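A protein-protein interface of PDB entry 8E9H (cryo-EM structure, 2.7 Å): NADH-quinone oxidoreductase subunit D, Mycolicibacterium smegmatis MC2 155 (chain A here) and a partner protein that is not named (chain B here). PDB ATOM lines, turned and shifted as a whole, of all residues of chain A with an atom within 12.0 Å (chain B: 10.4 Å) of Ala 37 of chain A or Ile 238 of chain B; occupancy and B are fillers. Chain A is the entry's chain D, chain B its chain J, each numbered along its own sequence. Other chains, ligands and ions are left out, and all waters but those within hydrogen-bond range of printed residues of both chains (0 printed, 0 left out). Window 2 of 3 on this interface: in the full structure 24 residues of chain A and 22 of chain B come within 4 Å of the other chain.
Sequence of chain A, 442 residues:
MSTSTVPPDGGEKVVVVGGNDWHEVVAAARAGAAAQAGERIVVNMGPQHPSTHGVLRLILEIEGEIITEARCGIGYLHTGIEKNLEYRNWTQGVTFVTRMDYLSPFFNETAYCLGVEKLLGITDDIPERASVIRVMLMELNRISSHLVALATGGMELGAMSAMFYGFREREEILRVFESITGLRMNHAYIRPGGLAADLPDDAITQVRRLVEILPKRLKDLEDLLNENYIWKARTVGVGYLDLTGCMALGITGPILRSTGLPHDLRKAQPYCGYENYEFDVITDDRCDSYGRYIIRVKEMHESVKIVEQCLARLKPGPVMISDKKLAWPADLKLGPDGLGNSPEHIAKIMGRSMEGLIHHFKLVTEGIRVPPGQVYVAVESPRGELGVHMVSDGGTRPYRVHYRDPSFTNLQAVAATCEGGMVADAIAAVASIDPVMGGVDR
The backbone carbonyl oxygen (O) of Leu 233 of chain B sits at hydrogen-bond distance from the guanidinium group (NH2) of Arg 71 of chain A, 2.8 Å away. The guanidinium group (NE) of Arg 71 of chain A is in hydrogen-bond range of the backbone carbonyl oxygen (O) of Ser 234 of chain B, 3.4 Å away. The side-chain hydroxyl of Ser 236 of chain B sits at hydrogen-bond distance from the side-chain carboxylate of Glu 61 of chain A (2.5 Å).
The guanidinium group (NH1) of Arg 40 of chain A is in salt-bridge range of the side-chain carboxylate (OE2) of Glu 61 of chain A. The backbone NH (N) of Ile 59 of chain A sits at hydrogen-bond distance from the backbone carbonyl oxygen (O) of Arg 71 of chain A, 2.9 Å away. O of Glu 61 of chain A is in hydrogen-bond range of N of Thr 68 of chain A (2.6 Å). The backbone NH (N) of Glu 61 of chain A sits at hydrogen-bond distance from the backbone carbonyl oxygen (O) of Glu 69 of chain A, at 2.9 Å. OE2 of Glu 69 of chain A is in salt-bridge range of NH1 of Arg 71 of chain A (2.6 Å).
Ala 37 of chain A touches Ile 238 of chain B. Ile 238 of chain B touches Arg 40 of chain A (CD1 to CB, 3.6 Å). Val 42 of chain A touches Val 219 of chain B. Val 42 of chain A touches Leu 239 of chain B (CG1 to CD2, 3.7 Å). Val 219 of chain B touches Asn 44 of chain A (CG1 to OD1, 2.9 Å). Ile 59 of chain A touches Val 219 of chain B (CG2 to CG1, 3.4 Å). CD1 of Ile 238 of chain B touches CD of Glu 61 of chain A, 3.6 Å away. Leu 207 of chain B touches Glu 69 of chain A (CD1 to CD, 3.3 Å). Leu 207 of chain B touches Arg 71 of chain A. Ser 236 of chain B touches Arg 71 of chain A.
Ala 37 of chain A touches one residue of chain B. No residue of chain B comes within 4 Å of Glu 39 of chain A. Printed residues of chain B within 4 Å of Glu 61 of chain A: Ser 236 and Ile 238. Printed residues of chain B within 4 Å of Glu 69 of chain A: Leu 207 (3.3 Å). Of the printed residues of chain A, Ser 236 of chain B touches Glu 61 and Arg 71. Leu 239 of chain B touches just one residue of chain A: Val 42. No residue of chain A comes within 4 Å of Pro 240 of chain B. The nearest residue of chain A that does not touch Ile 238 of chain B is Ile 41 of chain A (4.7 Å).
Of the 21 printed residues of chain A, 8 touch a printed residue of chain B. Printed residues of chain A that touch a printed residue of chain B: Ala 37, Arg 40, Val 42, Asn 44, Ile 59, Glu 61, Glu 69 and Arg 71. Hydrophobic or aromatic side chains of chain B that line the printed part of chain A: Leu 207, Val 219, Ile 238 and Leu 239. Along chain B the printed residues that touch a printed residue of chain A span positions 207 to 239. Among the printed residues, 13 pairs touch across the chains. Among the printed residues, no Asp or Glu carboxylate lies within 4 Å of a Lys or Arg side-chain nitrogen of the other chain.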
ATOM      1  N   GLN A  36      33.670 -14.523 -20.060  1.00  0.00           N
ATOM      2  CA  GLN A  36      33.540 -13.703 -21.257  1.00  0.00           C
ATOM      3  C   GLN A  36      32.788 -14.455 -22.347  1.00  0.00           C
ATOM      4  O   GLN A  36      32.152 -15.473 -22.086  1.00  0.00           O
ATOM      5  CB  GLN A  36      34.917 -13.277 -21.767  1.00  0.00           C
ATOM      6  N   ALA A  37      32.870 -13.946 -23.577  1.00  0.00           N
ATOM      7  CA  ALA A  37      32.140 -14.558 -24.682  1.00  0.00           C
ATOM      8  C   ALA A  37      32.614 -15.980 -24.943  1.00  0.00           C
ATOM      9  O   ALA A  37      31.806 -16.872 -25.223  1.00  0.00           O
ATOM     10  CB  ALA A  37      32.293 -13.707 -25.942  1.00  0.00           C
ATOM     11  N   GLY A  38      33.923 -16.213 -24.857  1.00  0.00           N
ATOM     12  CA  GLY A  38      34.459 -17.526 -25.162  1.00  0.00           C
ATOM     13  C   GLY A  38      33.902 -18.635 -24.296  1.00  0.00           C
ATOM     14  O   GLY A  38      33.875 -19.791 -24.729  1.00  0.00           O
ATOM     15  N   GLU A  39      33.450 -18.313 -23.088  1.00  0.00           N
ATOM     16  CA  GLU A  39      32.965 -19.312 -22.147  1.00  0.00           C
ATOM     17  C   GLU A  39      31.446 -19.425 -22.130  1.00  0.00           C
ATOM     18  O   GLU A  39      30.903 -20.152 -21.295  1.00  0.00           O
ATOM     19  CB  GLU A  39      33.473 -18.995 -20.741  1.00  0.00           C
ATOM     20  N   ARG A  40      30.751 -18.733 -23.027  1.00  0.00           N
ATOM     21  CA  ARG A  40      29.295 -18.710 -23.050  1.00  0.00           C
ATOM     22  C   ARG A  40      28.794 -19.368 -24.324  1.00  0.00           C
ATOM     23  O   ARG A  40      29.218 -18.996 -25.423  1.00  0.00           O
ATOM     24  CB  ARG A  40      28.770 -17.279 -22.968  1.00  0.00           C
ATOM     25  CG  ARG A  40      29.126 -16.549 -21.697  1.00  0.00           C
ATOM     26  CD  ARG A  40      28.218 -16.956 -20.562  1.00  0.00           C
ATOM     27  NE  ARG A  40      28.563 -16.273 -19.323  1.00  0.00           N
ATOM     28  CZ  ARG A  40      28.373 -14.978 -19.107  1.00  0.00           C
ATOM     29  NH1 ARG A  40      27.830 -14.196 -20.024  1.00  0.00           N
ATOM     30  NH2 ARG A  40      28.732 -14.458 -17.939  1.00  0.00           N
ATOM     31  N   ILE A  41      27.896 -20.337 -24.179  1.00  0.00           N
ATOM     32  CA  ILE A  41      27.131 -20.818 -25.318  1.00  0.00           C
ATOM     33  C   ILE A  41      25.786 -20.106 -25.343  1.00  0.00           C
ATOM     34  O   ILE A  41      25.291 -19.625 -24.326  1.00  0.00           O
ATOM     35  CB  ILE A  41      26.943 -22.343 -25.267  1.00  0.00           C
ATOM     36  CG1 ILE A  41      28.282 -23.063 -25.377  1.00  0.00           C
ATOM     37  CG2 ILE A  41      26.029 -22.796 -26.392  1.00  0.00           C
ATOM     38  CD1 ILE A  41      28.205 -24.523 -24.992  1.00  0.00           C
ATOM     39  N   VAL A  42      25.191 -20.026 -26.526  1.00  0.00           N
ATOM     40  CA  VAL A  42      23.806 -19.604 -26.670  1.00  0.00           C
ATOM     41  C   VAL A  42      23.073 -20.702 -27.423  1.00  0.00           C
ATOM     42  O   VAL A  42      23.446 -21.044 -28.549  1.00  0.00           O
ATOM     43  CB  VAL A  42      23.683 -18.250 -27.390  1.00  0.00           C
ATOM     44  CG1 VAL A  42      24.316 -18.309 -28.759  1.00  0.00           C
ATOM     45  CG2 VAL A  42      22.231 -17.844 -27.493  1.00  0.00           C
ATOM     46  N   VAL A  43      22.049 -21.262 -26.795  1.00  0.00           N
ATOM     47  CA  VAL A  43      21.384 -22.455 -27.299  1.00  0.00           C
ATOM     48  C   VAL A  43      19.890 -22.193 -27.353  1.00  0.00           C
ATOM     49  O   VAL A  43      19.316 -21.597 -26.438  1.00  0.00           O
ATOM     50  CB  VAL A  43      21.689 -23.682 -26.419  1.00  0.00           C
ATOM     51  CG1 VAL A  43      21.130 -23.486 -25.025  1.00  0.00           C
ATOM     52  CG2 VAL A  43      21.134 -24.943 -27.048  1.00  0.00           C
ATOM     53  N   ASN A  44      19.260 -22.644 -28.429  1.00  0.00           N
ATOM     54  CA  ASN A  44      17.811 -22.576 -28.549  1.00  0.00           C
ATOM     55  C   ASN A  44      17.209 -23.757 -27.807  1.00  0.00           C
ATOM     56  O   ASN A  44      17.270 -24.892 -28.285  1.00  0.00           O
ATOM     57  CB  ASN A  44      17.390 -22.598 -30.012  1.00  0.00           C
ATOM     58  CG  ASN A  44      17.968 -21.454 -30.797  1.00  0.00           C
ATOM     59  OD1 ASN A  44      17.351 -20.400 -30.921  1.00  0.00           O
ATOM     60  ND2 ASN A  44      19.165 -21.650 -31.329  1.00  0.00           N
ATOM     61  N   ILE A  59      15.528 -19.099 -25.769  1.00  0.00           N
ATOM     62  CA  ILE A  59      16.906 -18.862 -26.178  1.00  0.00           C
ATOM     63  C   ILE A  59      17.701 -18.583 -24.915  1.00  0.00           C
ATOM     64  O   ILE A  59      17.511 -17.543 -24.274  1.00  0.00           O
ATOM     65  CB  ILE A  59      17.021 -17.692 -27.165  1.00  0.00           C
ATOM     66  CG1 ILE A  59      16.110 -17.919 -28.369  1.00  0.00           C
ATOM     67  CG2 ILE A  59      18.456 -17.519 -27.616  1.00  0.00           C
ATOM     68  CD1 ILE A  59      14.793 -17.205 -28.266  1.00  0.00           C
ATOM     69  N   LEU A  60      18.583 -19.508 -24.551  1.00  0.00           N
ATOM     70  CA  LEU A  60      19.288 -19.453 -23.280  1.00  0.00           C
ATOM     71  C   LEU A  60      20.771 -19.251 -23.539  1.00  0.00           C
ATOM     72  O   LEU A  60      21.394 -20.038 -24.256  1.00  0.00           O
ATOM     73  CB  LEU A  60      19.056 -20.734 -22.480  1.00  0.00           C
ATOM     74  CG  LEU A  60      17.593 -21.086 -22.231  1.00  0.00           C
ATOM     75  CD1 LEU A  60      17.494 -22.362 -21.428  1.00  0.00           C
ATOM     76  CD2 LEU A  60      16.881 -19.956 -21.519  1.00  0.00           C
ATOM     77  N   GLU A  61      21.326 -18.194 -22.961  1.00  0.00           N
ATOM     78  CA  GLU A  61      22.768 -18.033 -22.895  1.00  0.00           C
ATOM     79  C   GLU A  61      23.261 -18.655 -21.600  1.00  0.00           C
ATOM     80  O   GLU A  61      22.871 -18.222 -20.511  1.00  0.00           O
ATOM     81  CB  GLU A  61      23.144 -16.556 -22.954  1.00  0.00           C
ATOM     82  CG  GLU A  61      24.634 -16.298 -22.957  1.00  0.00           C
ATOM     83  CD  GLU A  61      24.960 -14.828 -22.828  1.00  0.00           C
ATOM     84  OE1 GLU A  61      24.252 -14.004 -23.443  1.00  0.00           O
ATOM     85  OE2 GLU A  61      25.921 -14.494 -22.106  1.00  0.00           O
ATOM     86  N   ILE A  62      24.118 -19.665 -21.724  1.00  0.00           N
ATOM     87  CA  ILE A  62      24.542 -20.497 -20.608  1.00  0.00           C
ATOM     88  C   ILE A  62      26.058 -20.451 -20.497  1.00  0.00           C
ATOM     89  O   ILE A  62      26.769 -20.627 -21.494  1.00  0.00           O
ATOM     90  CB  ILE A  62      24.053 -21.948 -20.776  1.00  0.00           C
ATOM     91  CG1 ILE A  62      24.799 -22.637 -21.918  1.00  0.00           C
ATOM     92  CG2 ILE A  62      22.568 -21.972 -21.048  1.00  0.00           C
ATOM     93  CD1 ILE A  62      24.241 -23.990 -22.268  1.00  0.00           C
ATOM     94  N   GLU A  63      26.547 -20.208 -19.285  1.00  0.00           N
ATOM     95  CA  GLU A  63      27.960 -20.356 -18.950  1.00  0.00           C
ATOM     96  C   GLU A  63      28.097 -21.715 -18.277  1.00  0.00           C
ATOM     97  O   GLU A  63      27.673 -21.899 -17.136  1.00  0.00           O
ATOM     98  CB  GLU A  63      28.437 -19.228 -18.044  1.00  0.00           C
ATOM     99  N   GLY A  64      28.685 -22.670 -18.987  1.00  0.00           N
ATOM    100  CA  GLY A  64      28.681 -24.036 -18.511  1.00  0.00           C
ATOM    101  C   GLY A  64      27.297 -24.624 -18.660  1.00  0.00           C
ATOM    102  O   GLY A  64      26.857 -24.911 -19.776  1.00  0.00           O
ATOM    103  N   ILE A  66      24.827 -23.105 -16.358  1.00  0.00           N
ATOM    104  CA  ILE A  66      24.029 -22.114 -15.647  1.00  0.00           C
ATOM    105  C   ILE A  66      23.423 -21.157 -16.661  1.00  0.00           C
ATOM    106  O   ILE A  66      24.128 -20.625 -17.525  1.00  0.00           O
ATOM    107  CB  ILE A  66      24.891 -21.359 -14.625  1.00  0.00           C
ATOM    108  CG1 ILE A  66      25.222 -22.256 -13.435  1.00  0.00           C
ATOM    109  CG2 ILE A  66      24.181 -20.108 -14.158  1.00  0.00           C
ATOM    110  CD1 ILE A  66      24.075 -22.470 -12.480  1.00  0.00           C
ATOM    111  N   ILE A  67      22.116 -20.932 -16.561  1.00  0.00           N
ATOM    112  CA  ILE A  67      21.435 -20.044 -17.498  1.00  0.00           C
ATOM    113  C   ILE A  67      21.823 -18.611 -17.151  1.00  0.00           C
ATOM    114  O   ILE A  67      21.315 -18.039 -16.184  1.00  0.00           O
ATOM    115  CB  ILE A  67      19.916 -20.228 -17.450  1.00  0.00           C
ATOM    116  CG1 ILE A  67      19.537 -21.696 -17.637  1.00  0.00           C
ATOM    117  CG2 ILE A  67      19.256 -19.389 -18.523  1.00  0.00           C
ATOM    118  CD1 ILE A  67      20.178 -22.354 -18.830  1.00  0.00           C
ATOM    119  N   THR A  68      22.725 -18.028 -17.937  1.00  0.00           N
ATOM    120  CA  THR A  68      23.125 -16.647 -17.698  1.00  0.00           C
ATOM    121  C   THR A  68      22.072 -15.666 -18.192  1.00  0.00           C
ATOM    122  O   THR A  68      21.880 -14.606 -17.590  1.00  0.00           O
ATOM    123  CB  THR A  68      24.461 -16.361 -18.376  1.00  0.00           C
ATOM    124  OG1 THR A  68      25.450 -17.278 -17.894  1.00  0.00           O
ATOM    125  CG2 THR A  68      24.904 -14.940 -18.087  1.00  0.00           C
ATOM    126  N   GLU A  69      21.394 -15.994 -19.286  1.00  0.00           N
ATOM    127  CA  GLU A  69      20.411 -15.087 -19.860  1.00  0.00           C
ATOM    128  C   GLU A  69      19.318 -15.890 -20.542  1.00  0.00           C
ATOM    129  O   GLU A  69      19.559 -16.993 -21.033  1.00  0.00           O
ATOM    130  CB  GLU A  69      21.060 -14.133 -20.862  1.00  0.00           C
ATOM    131  CG  GLU A  69      20.227 -12.919 -21.182  1.00  0.00           C
ATOM    132  CD  GLU A  69      21.071 -11.754 -21.644  1.00  0.00           C
ATOM    133  OE1 GLU A  69      21.532 -10.976 -20.784  1.00  0.00           O
ATOM    134  OE2 GLU A  69      21.282 -11.622 -22.868  1.00  0.00           O
ATOM    135  N   ALA A  70      18.119 -15.316 -20.591  1.00  0.00           N
ATOM    136  CA  ALA A  70      16.965 -15.981 -21.174  1.00  0.00           C
ATOM    137  C   ALA A  70      16.182 -15.014 -22.048  1.00  0.00           C
ATOM    138  O   ALA A  70      15.986 -13.851 -21.688  1.00  0.00           O
ATOM    139  CB  ALA A  70      16.050 -16.549 -20.091  1.00  0.00           C
ATOM    140  N   ARG A  71      15.739 -15.509 -23.200  1.00  0.00           N
ATOM    141  CA  ARG A  71      14.834 -14.798 -24.086  1.00  0.00           C
ATOM    142  C   ARG A  71      13.776 -15.779 -24.561  1.00  0.00           C
ATOM    143  O   ARG A  71      13.996 -16.990 -24.549  1.00  0.00           O
ATOM    144  CB  ARG A  71      15.560 -14.213 -25.297  1.00  0.00           C
ATOM    145  CG  ARG A  71      16.660 -13.225 -24.975  1.00  0.00           C
ATOM    146  CD  ARG A  71      17.392 -12.823 -26.244  1.00  0.00           C
ATOM    147  NE  ARG A  71      18.114 -11.568 -26.095  1.00  0.00           N
ATOM    148  CZ  ARG A  71      19.231 -11.427 -25.396  1.00  0.00           C
ATOM    149  NH1 ARG A  71      19.787 -12.448 -24.768  1.00  0.00           N
ATOM    150  NH2 ARG A  71      19.806 -10.230 -25.327  1.00  0.00           N
ATOM    151  N   LEU B 207      14.671 -10.072 -22.248  1.00  0.00           N
ATOM    152  CA  LEU B 207      15.218  -9.279 -23.338  1.00  0.00           C
ATOM    153  C   LEU B 207      14.546  -9.687 -24.642  1.00  0.00           C
ATOM    154  O   LEU B 207      14.118 -10.838 -24.782  1.00  0.00           O
ATOM    155  CB  LEU B 207      16.731  -9.461 -23.426  1.00  0.00           C
ATOM    156  CG  LEU B 207      17.528  -8.812 -22.296  1.00  0.00           C
ATOM    157  CD1 LEU B 207      18.928  -9.378 -22.253  1.00  0.00           C
ATOM    158  CD2 LEU B 207      17.581  -7.308 -22.470  1.00  0.00           C
ATOM    159  N   VAL B 219      19.881 -17.515 -33.499  1.00  0.00           N
ATOM    160  CA  VAL B 219      19.929 -16.590 -32.373  1.00  0.00           C
ATOM    161  C   VAL B 219      20.820 -15.405 -32.716  1.00  0.00           C
ATOM    162  O   VAL B 219      20.785 -14.374 -32.039  1.00  0.00           O
ATOM    163  CB  VAL B 219      20.424 -17.291 -31.097  1.00  0.00           C
ATOM    164  CG1 VAL B 219      19.507 -18.438 -30.737  1.00  0.00           C
ATOM    165  CG2 VAL B 219      21.847 -17.777 -31.274  1.00  0.00           C
ATOM    166  N   ASP B 220      21.629 -15.544 -33.763  1.00  0.00           N
ATOM    167  CA  ASP B 220      22.522 -14.469 -34.170  1.00  0.00           C
ATOM    168  C   ASP B 220      21.776 -13.324 -34.837  1.00  0.00           C
ATOM    169  O   ASP B 220      22.236 -12.179 -34.797  1.00  0.00           O
ATOM    170  CB  ASP B 220      23.591 -15.009 -35.121  1.00  0.00           C
ATOM    171  N   PRO B 232      19.558  -3.593 -30.863  1.00  0.00           N
ATOM    172  CA  PRO B 232      20.766  -4.120 -30.207  1.00  0.00           C
ATOM    173  C   PRO B 232      20.469  -5.155 -29.141  1.00  0.00           C
ATOM    174  O   PRO B 232      21.209  -6.137 -29.015  1.00  0.00           O
ATOM    175  CB  PRO B 232      21.415  -2.863 -29.612  1.00  0.00           C
ATOM    176  CG  PRO B 232      20.823  -1.725 -30.365  1.00  0.00           C
ATOM    177  CD  PRO B 232      19.431  -2.139 -30.682  1.00  0.00           C
ATOM    178  N   LEU B 233      19.401  -4.967 -28.365  1.00  0.00           N
ATOM    179  CA  LEU B 233      19.104  -5.889 -27.278  1.00  0.00           C
ATOM    180  C   LEU B 233      18.657  -7.253 -27.778  1.00  0.00           C
ATOM    181  O   LEU B 233      18.737  -8.230 -27.029  1.00  0.00           O
ATOM    182  CB  LEU B 233      18.018  -5.303 -26.377  1.00  0.00           C
ATOM    183  CG  LEU B 233      18.363  -4.002 -25.653  1.00  0.00           C
ATOM    184  CD1 LEU B 233      17.189  -3.550 -24.808  1.00  0.00           C
ATOM    185  CD2 LEU B 233      19.601  -4.169 -24.794  1.00  0.00           C
ATOM    186  N   SER B 234      18.187  -7.341 -29.021  1.00  0.00           N
ATOM    187  CA  SER B 234      17.603  -8.584 -29.504  1.00  0.00           C
ATOM    188  C   SER B 234      18.608  -9.722 -29.561  1.00  0.00           C
ATOM    189  O   SER B 234      18.213 -10.883 -29.421  1.00  0.00           O
ATOM    190  CB  SER B 234      16.998  -8.366 -30.887  1.00  0.00           C
ATOM    191  OG  SER B 234      18.009  -8.136 -31.847  1.00  0.00           O
ATOM    192  N   VAL B 235      19.890  -9.426 -29.751  1.00  0.00           N
ATOM    193  CA  VAL B 235      20.919 -10.446 -29.894  1.00  0.00           C
ATOM    194  C   VAL B 235      21.930 -10.269 -28.775  1.00  0.00           C
ATOM    195  O   VAL B 235      22.351  -9.144 -28.483  1.00  0.00           O
ATOM    196  CB  VAL B 235      21.611 -10.370 -31.268  1.00  0.00           C
ATOM    197  CG1 VAL B 235      22.361  -9.059 -31.415  1.00  0.00           C
ATOM    198  CG2 VAL B 235      22.548 -11.545 -31.449  1.00  0.00           C
ATOM    199  N   SER B 236      22.316 -11.375 -28.147  1.00  0.00           N
ATOM    200  CA  SER B 236      23.262 -11.315 -27.043  1.00  0.00           C
ATOM    201  C   SER B 236      24.569 -10.679 -27.494  1.00  0.00           C
ATOM    202  O   SER B 236      25.048 -10.922 -28.604  1.00  0.00           O
ATOM    203  CB  SER B 236      23.523 -12.714 -26.492  1.00  0.00           C
ATOM    204  OG  SER B 236      24.528 -12.681 -25.495  1.00  0.00           O
ATOM    205  N   THR B 237      25.150  -9.861 -26.617  1.00  0.00           N
ATOM    206  CA  THR B 237      26.362  -9.134 -26.971  1.00  0.00           C
ATOM    207  C   THR B 237      27.520 -10.064 -27.297  1.00  0.00           C
ATOM    208  O   THR B 237      28.397  -9.690 -28.083  1.00  0.00           O
ATOM    209  CB  THR B 237      26.765  -8.201 -25.831  1.00  0.00           C
ATOM    210  OG1 THR B 237      26.971  -8.965 -24.637  1.00  0.00           O
ATOM    211  CG2 THR B 237      25.683  -7.168 -25.584  1.00  0.00           C
ATOM    212  N   ILE B 238      27.548 -11.264 -26.715  1.00  0.00           N
ATOM    213  CA  ILE B 238      28.666 -12.166 -26.963  1.00  0.00           C
ATOM    214  C   ILE B 238      28.738 -12.543 -28.435  1.00  0.00           C
ATOM    215  O   ILE B 238      29.832 -12.672 -28.997  1.00  0.00           O
ATOM    216  CB  ILE B 238      28.556 -13.410 -26.062  1.00  0.00           C
ATOM    217  CG1 ILE B 238      27.385 -14.293 -26.497  1.00  0.00           C
ATOM    218  CG2 ILE B 238      28.396 -12.997 -24.609  1.00  0.00           C
ATOM    219  CD1 ILE B 238      27.191 -15.511 -25.631  1.00  0.00           C
ATOM    220  N   LEU B 239      27.600 -12.722 -29.081  1.00  0.00           N
ATOM    221  CA  LEU B 239      27.607 -13.122 -30.478  1.00  0.00           C
ATOM    222  C   LEU B 239      28.154 -11.995 -31.351  1.00  0.00           C
ATOM    223  O   LEU B 239      27.916 -10.818 -31.065  1.00  0.00           O
ATOM    224  CB  LEU B 239      26.201 -13.481 -30.939  1.00  0.00           C
ATOM    225  CG  LEU B 239      25.591 -14.713 -30.282  1.00  0.00           C
ATOM    226  CD1 LEU B 239      24.078 -14.637 -30.332  1.00  0.00           C
ATOM    227  CD2 LEU B 239      26.099 -15.959 -30.976  1.00  0.00           C
ATOM    228  N   PRO B 240      28.886 -12.321 -32.416  1.00  0.00           N
ATOM    229  CA  PRO B 240      29.266 -11.285 -33.385  1.00  0.00           C
ATOM    230  C   PRO B 240      28.085 -10.886 -34.252  1.00  0.00           C
ATOM    231  O   PRO B 240      27.458 -11.744 -34.878  1.00  0.00           O
ATOM    232  CB  PRO B 240      30.370 -11.960 -34.202  1.00  0.00           C
ATOM    233  CG  PRO B 240      30.041 -13.406 -34.133  1.00  0.00           C
ATOM    234  CD  PRO B 240      29.458 -13.632 -32.766  1.00  0.00           C
ATOM    235  N   HIS B 241      27.767  -9.596 -34.290  1.00  0.00           N
ATOM    236  CA  HIS B 241      26.617  -9.117 -35.045  1.00  0.00           C
ATOM    237  C   HIS B 241      26.694  -9.570 -36.494  1.00  0.00           C
ATOM    238  O   HIS B 241      27.551  -9.112 -37.258  1.00  0.00           O
ATOM    239  CB  HIS B 241      26.551  -7.589 -34.972  1.00  0.00           C
ATOM    240  N   ARG B 242      25.796 -10.477 -36.874  1.00  0.00           N
ATOM    241  CA  ARG B 242      25.776 -11.016 -38.228  1.00  0.00           C
ATOM    242  C   ARG B 242      24.486 -11.787 -38.477  1.00  0.00           C
ATOM    243  O   ARG B 242      23.565 -11.749 -37.656  1.00  0.00           O
ATOM    244  CB  ARG B 242      26.989 -11.916 -38.466  1.00  0.00           C
